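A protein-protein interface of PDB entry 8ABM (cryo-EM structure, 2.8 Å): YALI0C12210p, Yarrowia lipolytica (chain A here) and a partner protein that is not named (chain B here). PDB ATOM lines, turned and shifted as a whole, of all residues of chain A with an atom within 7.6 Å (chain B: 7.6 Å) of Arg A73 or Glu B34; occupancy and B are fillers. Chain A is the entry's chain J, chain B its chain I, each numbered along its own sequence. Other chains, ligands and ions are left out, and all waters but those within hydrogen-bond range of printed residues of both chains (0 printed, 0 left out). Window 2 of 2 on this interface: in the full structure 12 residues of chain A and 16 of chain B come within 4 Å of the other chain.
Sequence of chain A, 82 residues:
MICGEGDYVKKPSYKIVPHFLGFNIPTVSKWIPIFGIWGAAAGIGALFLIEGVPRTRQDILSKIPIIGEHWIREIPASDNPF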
ATOM      1  N   GLU A  51     -16.132   1.049 -29.977  1.00  0.00           N
ATOM      2  CA  GLU A  51     -15.017   0.228 -30.404  1.00  0.00           C
ATOM      3  C   GLU A  51     -15.224  -1.187 -29.869  1.00  0.00           C
ATOM      4  O   GLU A  51     -14.779  -2.156 -30.471  1.00  0.00           O
ATOM      5  CB  GLU A  51     -13.732   0.878 -29.889  1.00  0.00           C
ATOM      6  CG  GLU A  51     -12.466   0.042 -30.066  1.00  0.00           C
ATOM      7  CD  GLU A  51     -12.166  -1.065 -29.061  1.00  0.00           C
ATOM      8  OE1 GLU A  51     -12.509  -0.908 -27.865  1.00  0.00           O
ATOM      9  OE2 GLU A  51     -11.566  -2.088 -29.469  1.00  0.00           O
ATOM     10  N   GLY A  52     -15.876  -1.285 -28.709  1.00  0.00           N
ATOM     11  CA  GLY A  52     -16.082  -2.561 -28.051  1.00  0.00           C
ATOM     12  C   GLY A  52     -17.166  -3.408 -28.716  1.00  0.00           C
ATOM     13  O   GLY A  52     -17.068  -4.632 -28.709  1.00  0.00           O
ATOM     14  N   ARG A  57     -16.097  -3.879 -34.836  1.00  0.00           N
ATOM     15  CA  ARG A  57     -14.779  -4.424 -35.100  1.00  0.00           C
ATOM     16  C   ARG A  57     -14.838  -5.163 -36.423  1.00  0.00           C
ATOM     17  O   ARG A  57     -14.014  -4.931 -37.302  1.00  0.00           O
ATOM     18  CB  ARG A  57     -14.362  -5.360 -33.972  1.00  0.00           C
ATOM     19  CG  ARG A  57     -14.455  -4.701 -32.613  1.00  0.00           C
ATOM     20  CD  ARG A  57     -13.985  -5.589 -31.518  1.00  0.00           C
ATOM     21  NE  ARG A  57     -13.728  -4.800 -30.328  1.00  0.00           N
ATOM     22  CZ  ARG A  57     -13.306  -5.348 -29.206  1.00  0.00           C
ATOM     23  NH1 ARG A  57     -13.127  -6.657 -29.156  1.00  0.00           N
ATOM     24  NH2 ARG A  57     -13.061  -4.608 -28.141  1.00  0.00           N
ATOM     25  N   SER A  62     -11.561  -3.818 -38.248  1.00  0.00           N
ATOM     26  CA  SER A  62     -10.679  -4.890 -38.682  1.00  0.00           C
ATOM     27  C   SER A  62     -10.276  -4.727 -40.147  1.00  0.00           C
ATOM     28  O   SER A  62      -9.383  -5.431 -40.624  1.00  0.00           O
ATOM     29  CB  SER A  62     -11.281  -6.237 -38.414  1.00  0.00           C
ATOM     30  OG  SER A  62     -12.439  -6.436 -39.210  1.00  0.00           O
ATOM     31  N   GLY A  68      -5.507  -3.125 -38.585  1.00  0.00           N
ATOM     32  CA  GLY A  68      -6.771  -3.841 -38.492  1.00  0.00           C
ATOM     33  C   GLY A  68      -6.700  -5.223 -37.844  1.00  0.00           C
ATOM     34  O   GLY A  68      -7.726  -5.760 -37.436  1.00  0.00           O
ATOM     35  N   GLU A  69      -5.502  -5.809 -37.751  1.00  0.00           N
ATOM     36  CA  GLU A  69      -5.380  -7.138 -37.173  1.00  0.00           C
ATOM     37  C   GLU A  69      -5.494  -7.074 -35.655  1.00  0.00           C
ATOM     38  O   GLU A  69      -5.643  -8.104 -35.007  1.00  0.00           O
ATOM     39  CB  GLU A  69      -4.050  -7.769 -37.560  1.00  0.00           C
ATOM     40  CG  GLU A  69      -3.964  -8.105 -39.034  1.00  0.00           C
ATOM     41  CD  GLU A  69      -2.597  -7.863 -39.647  1.00  0.00           C
ATOM     42  OE1 GLU A  69      -1.595  -8.331 -39.064  1.00  0.00           O
ATOM     43  OE2 GLU A  69      -2.531  -7.198 -40.706  1.00  0.00           O
ATOM     44  N   HIS A  70      -5.391  -5.861 -35.102  1.00  0.00           N
ATOM     45  CA  HIS A  70      -5.548  -5.642 -33.675  1.00  0.00           C
ATOM     46  C   HIS A  70      -6.916  -6.145 -33.210  1.00  0.00           C
ATOM     47  O   HIS A  70      -7.068  -6.544 -32.057  1.00  0.00           O
ATOM     48  CB  HIS A  70      -5.271  -4.172 -33.319  1.00  0.00           C
ATOM     49  CG  HIS A  70      -5.576  -3.831 -31.899  1.00  0.00           C
ATOM     50  ND1 HIS A  70      -4.711  -4.124 -30.862  1.00  0.00           N
ATOM     51  CD2 HIS A  70      -6.663  -3.262 -31.336  1.00  0.00           C
ATOM     52  CE1 HIS A  70      -5.256  -3.742 -29.723  1.00  0.00           C
ATOM     53  NE2 HIS A  70      -6.454  -3.209 -29.987  1.00  0.00           N
ATOM     54  N   TRP A  71      -7.900  -6.137 -34.119  1.00  0.00           N
ATOM     55  CA  TRP A  71      -9.282  -6.404 -33.753  1.00  0.00           C
ATOM     56  C   TRP A  71      -9.767  -7.761 -34.257  1.00  0.00           C
ATOM     57  O   TRP A  71     -10.938  -8.104 -34.080  1.00  0.00           O
ATOM     58  CB  TRP A  71     -10.184  -5.283 -34.258  1.00  0.00           C
ATOM     59  CG  TRP A  71     -10.009  -4.004 -33.506  1.00  0.00           C
ATOM     60  CD1 TRP A  71     -10.504  -3.689 -32.275  1.00  0.00           C
ATOM     61  CD2 TRP A  71      -9.265  -2.861 -33.941  1.00  0.00           C
ATOM     62  NE1 TRP A  71     -10.132  -2.420 -31.919  1.00  0.00           N
ATOM     63  CE2 TRP A  71      -9.367  -1.890 -32.918  1.00  0.00           C
ATOM     64  CE3 TRP A  71      -8.521  -2.574 -35.087  1.00  0.00           C
ATOM     65  CZ2 TRP A  71      -8.773  -0.637 -33.022  1.00  0.00           C
ATOM     66  CZ3 TRP A  71      -7.940  -1.332 -35.193  1.00  0.00           C
ATOM     67  CH2 TRP A  71      -8.055  -0.386 -34.170  1.00  0.00           C
ATOM     68  N   ILE A  72      -8.874  -8.525 -34.894  1.00  0.00           N
ATOM     69  CA  ILE A  72      -9.209  -9.878 -35.304  1.00  0.00           C
ATOM     70  C   ILE A  72      -8.611 -10.823 -34.266  1.00  0.00           C
ATOM     71  O   ILE A  72      -7.439 -11.185 -34.346  1.00  0.00           O
ATOM     72  CB  ILE A  72      -8.737 -10.186 -36.743  1.00  0.00           C
ATOM     73  CG1 ILE A  72      -9.078  -9.068 -37.736  1.00  0.00           C
ATOM     74  CG2 ILE A  72      -9.298 -11.526 -37.192  1.00  0.00           C
ATOM     75  CD1 ILE A  72      -8.170  -8.988 -38.959  1.00  0.00           C
ATOM     76  N   ARG A  73      -9.425 -11.183 -33.273  1.00  0.00           N
ATOM     77  CA  ARG A  73      -8.972 -12.031 -32.183  1.00  0.00           C
ATOM     78  C   ARG A  73      -9.978 -13.156 -31.965  1.00  0.00           C
ATOM     79  O   ARG A  73     -11.174 -12.900 -31.804  1.00  0.00           O
ATOM     80  CB  ARG A  73      -8.699 -11.217 -30.912  1.00  0.00           C
ATOM     81  CG  ARG A  73      -9.633 -10.033 -30.712  1.00  0.00           C
ATOM     82  CD  ARG A  73      -9.596  -9.475 -29.306  1.00  0.00           C
ATOM     83  NE  ARG A  73      -9.958  -8.062 -29.336  1.00  0.00           N
ATOM     84  CZ  ARG A  73      -9.114  -7.044 -29.169  1.00  0.00           C
ATOM     85  NH1 ARG A  73      -7.831  -7.275 -28.942  1.00  0.00           N
ATOM     86  NH2 ARG A  73      -9.555  -5.799 -29.229  1.00  0.00           N
ATOM     87  N   GLU A  74      -9.466 -14.395 -31.962  1.00  0.00           N
ATOM     88  CA  GLU A  74     -10.257 -15.598 -31.749  1.00  0.00           C
ATOM     89  C   GLU A  74      -9.897 -16.226 -30.407  1.00  0.00           C
ATOM     90  O   GLU A  74      -8.720 -16.374 -30.071  1.00  0.00           O
ATOM     91  CB  GLU A  74     -10.016 -16.624 -32.862  1.00  0.00           C
ATOM     92  CG  GLU A  74     -10.711 -16.292 -34.179  1.00  0.00           C
ATOM     93  CD  GLU A  74      -9.872 -15.646 -35.274  1.00  0.00           C
ATOM     94  OE1 GLU A  74      -8.728 -16.102 -35.497  1.00  0.00           O
ATOM     95  OE2 GLU A  74     -10.375 -14.701 -35.926  1.00  0.00           O
ATOM     96  N   ILE A  75     -10.940 -16.601 -29.657  1.00  0.00           N
ATOM     97  CA  ILE A  75     -10.805 -17.495 -28.519  1.00  0.00           C
ATOM     98  C   ILE A  75     -10.538 -18.894 -29.078  1.00  0.00           C
ATOM     99  O   ILE A  75     -11.281 -19.348 -29.952  1.00  0.00           O
ATOM    100  CB  ILE A  75     -12.061 -17.458 -27.614  1.00  0.00           C
ATOM    101  CG1 ILE A  75     -12.471 -16.037 -27.193  1.00  0.00           C
ATOM    102  CG2 ILE A  75     -11.921 -18.398 -26.420  1.00  0.00           C
ATOM    103  CD1 ILE A  75     -11.577 -15.364 -26.156  1.00  0.00           C
ATOM    104  N   PRO A  76      -9.467 -19.604 -28.629  1.00  0.00           N
ATOM    105  CA  PRO A  76      -9.213 -20.986 -29.054  1.00  0.00           C
ATOM    106  C   PRO A  76     -10.404 -21.861 -28.677  1.00  0.00           C
ATOM    107  O   PRO A  76     -10.959 -21.691 -27.600  1.00  0.00           O
ATOM    108  CB  PRO A  76      -7.981 -21.437 -28.246  1.00  0.00           C
ATOM    109  CG  PRO A  76      -7.337 -20.152 -27.763  1.00  0.00           C
ATOM    110  CD  PRO A  76      -8.438 -19.111 -27.697  1.00  0.00           C
ATOM    111  N   VAL B  28      -5.740   5.993 -29.204  1.00  0.00           N
ATOM    112  CA  VAL B  28      -4.470   5.309 -29.365  1.00  0.00           C
ATOM    113  C   VAL B  28      -3.987   4.813 -28.007  1.00  0.00           C
ATOM    114  O   VAL B  28      -3.539   3.677 -27.888  1.00  0.00           O
ATOM    115  CB  VAL B  28      -3.436   6.219 -30.042  1.00  0.00           C
ATOM    116  CG1 VAL B  28      -2.029   5.667 -29.913  1.00  0.00           C
ATOM    117  CG2 VAL B  28      -3.793   6.457 -31.494  1.00  0.00           C
ATOM    118  N   PHE B  29      -4.095   5.666 -26.989  1.00  0.00           N
ATOM    119  CA  PHE B  29      -3.676   5.273 -25.660  1.00  0.00           C
ATOM    120  C   PHE B  29      -4.460   4.040 -25.223  1.00  0.00           C
ATOM    121  O   PHE B  29      -3.872   3.040 -24.831  1.00  0.00           O
ATOM    122  CB  PHE B  29      -3.895   6.415 -24.673  1.00  0.00           C
ATOM    123  CG  PHE B  29      -3.657   5.989 -23.253  1.00  0.00           C
ATOM    124  CD1 PHE B  29      -2.363   5.907 -22.755  1.00  0.00           C
ATOM    125  CD2 PHE B  29      -4.713   5.624 -22.429  1.00  0.00           C
ATOM    126  CE1 PHE B  29      -2.132   5.502 -21.447  1.00  0.00           C
ATOM    127  CE2 PHE B  29      -4.481   5.213 -21.122  1.00  0.00           C
ATOM    128  CZ  PHE B  29      -3.192   5.152 -20.634  1.00  0.00           C
ATOM    129  N   ASP B  30      -5.787   4.110 -25.330  1.00  0.00           N
ATOM    130  CA  ASP B  30      -6.655   3.006 -24.953  1.00  0.00           C
ATOM    131  C   ASP B  30      -6.188   1.685 -25.568  1.00  0.00           C
ATOM    132  O   ASP B  30      -6.175   0.674 -24.876  1.00  0.00           O
ATOM    133  CB  ASP B  30      -8.103   3.299 -25.336  1.00  0.00           C
ATOM    134  CG  ASP B  30      -9.122   2.534 -24.506  1.00  0.00           C
ATOM    135  OD1 ASP B  30      -9.318   2.910 -23.325  1.00  0.00           O
ATOM    136  OD2 ASP B  30      -9.726   1.577 -25.041  1.00  0.00           O
ATOM    137  N   MET B  31      -5.844   1.690 -26.862  1.00  0.00           N
ATOM    138  CA  MET B  31      -5.521   0.476 -27.597  1.00  0.00           C
ATOM    139  C   MET B  31      -4.160  -0.071 -27.180  1.00  0.00           C
ATOM    140  O   MET B  31      -3.980  -1.279 -27.024  1.00  0.00           O
ATOM    141  CB  MET B  31      -5.514   0.734 -29.108  1.00  0.00           C
ATOM    142  CG  MET B  31      -6.894   0.946 -29.694  1.00  0.00           C
ATOM    143  SD  MET B  31      -8.089  -0.306 -29.154  1.00  0.00           S
ATOM    144  CE  MET B  31      -9.005   0.624 -27.927  1.00  0.00           C
ATOM    145  N   THR B  32      -3.206   0.835 -27.025  1.00  0.00           N
ATOM    146  CA  THR B  32      -1.838   0.438 -26.786  1.00  0.00           C
ATOM    147  C   THR B  32      -1.679   0.063 -25.325  1.00  0.00           C
ATOM    148  O   THR B  32      -0.934  -0.856 -25.025  1.00  0.00           O
ATOM    149  CB  THR B  32      -0.867   1.542 -27.197  1.00  0.00           C
ATOM    150  OG1 THR B  32      -1.309   2.727 -26.540  1.00  0.00           O
ATOM    151  CG2 THR B  32      -0.863   1.736 -28.694  1.00  0.00           C
ATOM    152  N   PHE B  33      -2.401   0.755 -24.442  1.00  0.00           N
ATOM    153  CA  PHE B  33      -2.266   0.514 -23.016  1.00  0.00           C
ATOM    154  C   PHE B  33      -2.817  -0.865 -22.684  1.00  0.00           C
ATOM    155  O   PHE B  33      -2.257  -1.568 -21.845  1.00  0.00           O
ATOM    156  CB  PHE B  33      -2.987   1.616 -22.242  1.00  0.00           C
ATOM    157  CG  PHE B  33      -2.930   1.520 -20.742  1.00  0.00           C
ATOM    158  CD1 PHE B  33      -1.716   1.560 -20.067  1.00  0.00           C
ATOM    159  CD2 PHE B  33      -4.102   1.469 -19.999  1.00  0.00           C
ATOM    160  CE1 PHE B  33      -1.674   1.504 -18.680  1.00  0.00           C
ATOM    161  CE2 PHE B  33      -4.061   1.415 -18.612  1.00  0.00           C
ATOM    162  CZ  PHE B  33      -2.846   1.433 -17.955  1.00  0.00           C
ATOM    163  N   GLU B  34      -3.918  -1.215 -23.354  1.00  0.00           N
ATOM    164  CA  GLU B  34      -4.548  -2.519 -23.251  1.00  0.00           C
ATOM    165  C   GLU B  34      -3.503  -3.587 -23.560  1.00  0.00           C
ATOM    166  O   GLU B  34      -3.303  -4.498 -22.767  1.00  0.00           O
ATOM    167  CB  GLU B  34      -5.747  -2.567 -24.204  1.00  0.00           C
ATOM    168  CG  GLU B  34      -6.590  -3.833 -24.119  1.00  0.00           C
ATOM    169  CD  GLU B  34      -6.439  -4.856 -25.240  1.00  0.00           C
ATOM    170  OE1 GLU B  34      -7.268  -5.796 -25.295  1.00  0.00           O
ATOM    171  OE2 GLU B  34      -5.494  -4.724 -26.053  1.00  0.00           O
ATOM    172  N   THR B  35      -2.851  -3.452 -24.717  1.00  0.00           N
ATOM    173  CA  THR B  35      -1.877  -4.412 -25.197  1.00  0.00           C
ATOM    174  C   THR B  35      -0.687  -4.497 -24.253  1.00  0.00           C
ATOM    175  O   THR B  35      -0.173  -5.586 -24.022  1.00  0.00           O
ATOM    176  CB  THR B  35      -1.426  -4.027 -26.605  1.00  0.00           C
ATOM    177  OG1 THR B  35      -2.590  -4.313 -27.376  1.00  0.00           O
ATOM    178  CG2 THR B  35      -0.242  -4.829 -27.102  1.00  0.00           C
ATOM    179  N   ALA B  36      -0.239  -3.350 -23.735  1.00  0.00           N
ATOM    180  CA  ALA B  36       0.954  -3.286 -22.902  1.00  0.00           C
ATOM    181  C   ALA B  36       0.697  -3.946 -21.552  1.00  0.00           C
ATOM    182  O   ALA B  36       1.574  -4.630 -21.026  1.00  0.00           O
ATOM    183  CB  ALA B  36       1.411  -1.857 -22.735  1.00  0.00           C
ATOM    184  N   ILE B  37      -0.507  -3.729 -21.008  1.00  0.00           N
ATOM    185  CA  ILE B  37      -0.822  -4.282 -19.704  1.00  0.00           C
ATOM    186  C   ILE B  37      -0.978  -5.786 -19.853  1.00  0.00           C
ATOM    187  O   ILE B  37      -0.406  -6.526 -19.061  1.00  0.00           O
ATOM    188  CB  ILE B  37      -2.021  -3.581 -19.023  1.00  0.00           C
ATOM    189  CG1 ILE B  37      -1.643  -2.180 -18.534  1.00  0.00           C
ATOM    190  CG2 ILE B  37      -2.613  -4.418 -17.892  1.00  0.00           C
ATOM    191  CD1 ILE B  37      -0.377  -2.122 -17.689  1.00  0.00           C
ATOM    192  N   ASP B  38      -1.694  -6.208 -20.903  1.00  0.00           N
ATOM    193  CA  ASP B  38      -1.847  -7.620 -21.206  1.00  0.00           C
ATOM    194  C   ASP B  38      -0.490  -8.319 -21.157  1.00  0.00           C
ATOM    195  O   ASP B  38      -0.372  -9.336 -20.487  1.00  0.00           O
ATOM    196  CB  ASP B  38      -2.525  -7.888 -22.554  1.00  0.00           C
ATOM    197  CG  ASP B  38      -4.018  -7.595 -22.627  1.00  0.00           C
ATOM    198  OD1 ASP B  38      -4.613  -7.242 -21.588  1.00  0.00           O
ATOM    199  OD2 ASP B  38      -4.579  -7.708 -23.743  1.00  0.00           O
ATOM    200  N   ASN B  39       0.524  -7.781 -21.853  1.00  0.00           N
ATOM    201  CA  ASN B  39       1.804  -8.474 -21.930  1.00  0.00           C
ATOM    202  C   ASN B  39       2.493  -8.469 -20.571  1.00  0.00           C
ATOM    203  O   ASN B  39       3.185  -9.419 -20.216  1.00  0.00           O
ATOM    204  CB  ASN B  39       2.726  -7.948 -23.032  1.00  0.00           C
ATOM    205  CG  ASN B  39       2.119  -8.083 -24.411  1.00  0.00           C
ATOM    206  OD1 ASN B  39       1.482  -9.088 -24.726  1.00  0.00           O
ATOM    207  ND2 ASN B  39       2.290  -7.063 -25.235  1.00  0.00           N
ATOM    208  N   PHE B  40       2.316  -7.382 -19.832  1.00  0.00           N
ATOM    209  CA  PHE B  40       3.024  -7.258 -18.580  1.00  0.00           C
ATOM    210  C   PHE B  40       2.445  -8.252 -17.583  1.00  0.00           C
ATOM    211  O   PHE B  40       3.176  -8.887 -16.830  1.00  0.00           O
ATOM    212  CB  PHE B  40       2.905  -5.823 -18.084  1.00  0.00           C
ATOM    213  CG  PHE B  40       3.403  -5.602 -16.683  1.00  0.00           C
ATOM    214  CD1 PHE B  40       4.763  -5.632 -16.392  1.00  0.00           C
ATOM    215  CD2 PHE B  40       2.507  -5.342 -15.656  1.00  0.00           C
ATOM    216  CE1 PHE B  40       5.213  -5.422 -15.095  1.00  0.00           C
ATOM    217  CE2 PHE B  40       2.958  -5.123 -14.360  1.00  0.00           C
ATOM    218  CZ  PHE B  40       4.309  -5.171 -14.080  1.00  0.00           C
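SD of Met B31 lies within hydrogen-bond range of NE2 of His A70 (3.4 Å).
OE1 of Glu B34 is in salt-bridge range of NH1 of Arg A73 (3.98 Å).
Of the printed residues of chain B, His A70 touches Met B31 (3.4 Å), Glu B34 (3.8 Å) and Thr B35 (3.6 Å).
Of the printed residues of chain B, Trp A71 touches Met B31 (3.9 Å).
Arg A73 touches just one residue of chain B: Glu B34.
Printed residues of chain A within 4 Å of Met B31: Glu A51, His A70 and Trp A71.
Of the printed residues of chain A, Glu B34 touches His A70 (3.8 Å) and Arg A73 (3.98 Å).
Of the printed residues of chain A, Thr B35 touches His A70 (3.6 Å).
The nearest residue of chain B that does not touch Arg A73 is Met B31 (5.7 Å).
The nearest residue of chain A that does not touch Glu B34 is Arg A57 (6.6 Å).
The nearest printed residue of chain A that does not touch Thr B35 is Arg A73 (6.2 Å).
Among the printed residues, merely in contact across the chains: His A70 with Thr B35, Glu A51 with Met B31, His A70 with Glu B34 and Trp A71 with Met B31.
NH2 of Arg A57 lies within salt-bridge range of OE2 of Glu A51 (3.2 Å).
NE1 of Trp A71 is in hydrogen-bond range of OE2 of Glu A51, 2.9 Å away.
The guanidinium group of Arg A73 lies within hydrogen-bond range of the backbone carbonyl oxygen of His A70, 3.3 Å away.
The backbone carbonyl oxygen of Met B31 is in hydrogen-bond range of the side-chain hydroxyl of Thr B35 (3.4 Å).
The side-chain carboxylate (OE2) of Glu B34 lies within hydrogen-bond range of the side-chain hydroxyl (OG1) of Thr B35 (3.2 Å).
The backbone carbonyl oxygen (O) of Thr B35 lies within hydrogen-bond range of the side-chain amide nitrogen (ND2) of Asn B39.
Of the 13 printed residues of chain B, 3 touch a printed residue of chain A.
Hydrophobic or aromatic side chains of chain B within 4 Å of the printed part of chain A: Met B31.
Of the 13 printed residues of chain A, 4 touch a printed residue of chain B.
Hydrophobic or aromatic side chains of chain A that line the printed part of chain B: His A70 and Trp A71.
Among the printed residues, 6 pairs touch across the chains.
Among the printed residues, Asp or Glu carboxylates within 4 Å of a Lys or Arg side-chain nitrogen of the other chain: Arg A73 with Glu B34 (3.98 Å).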
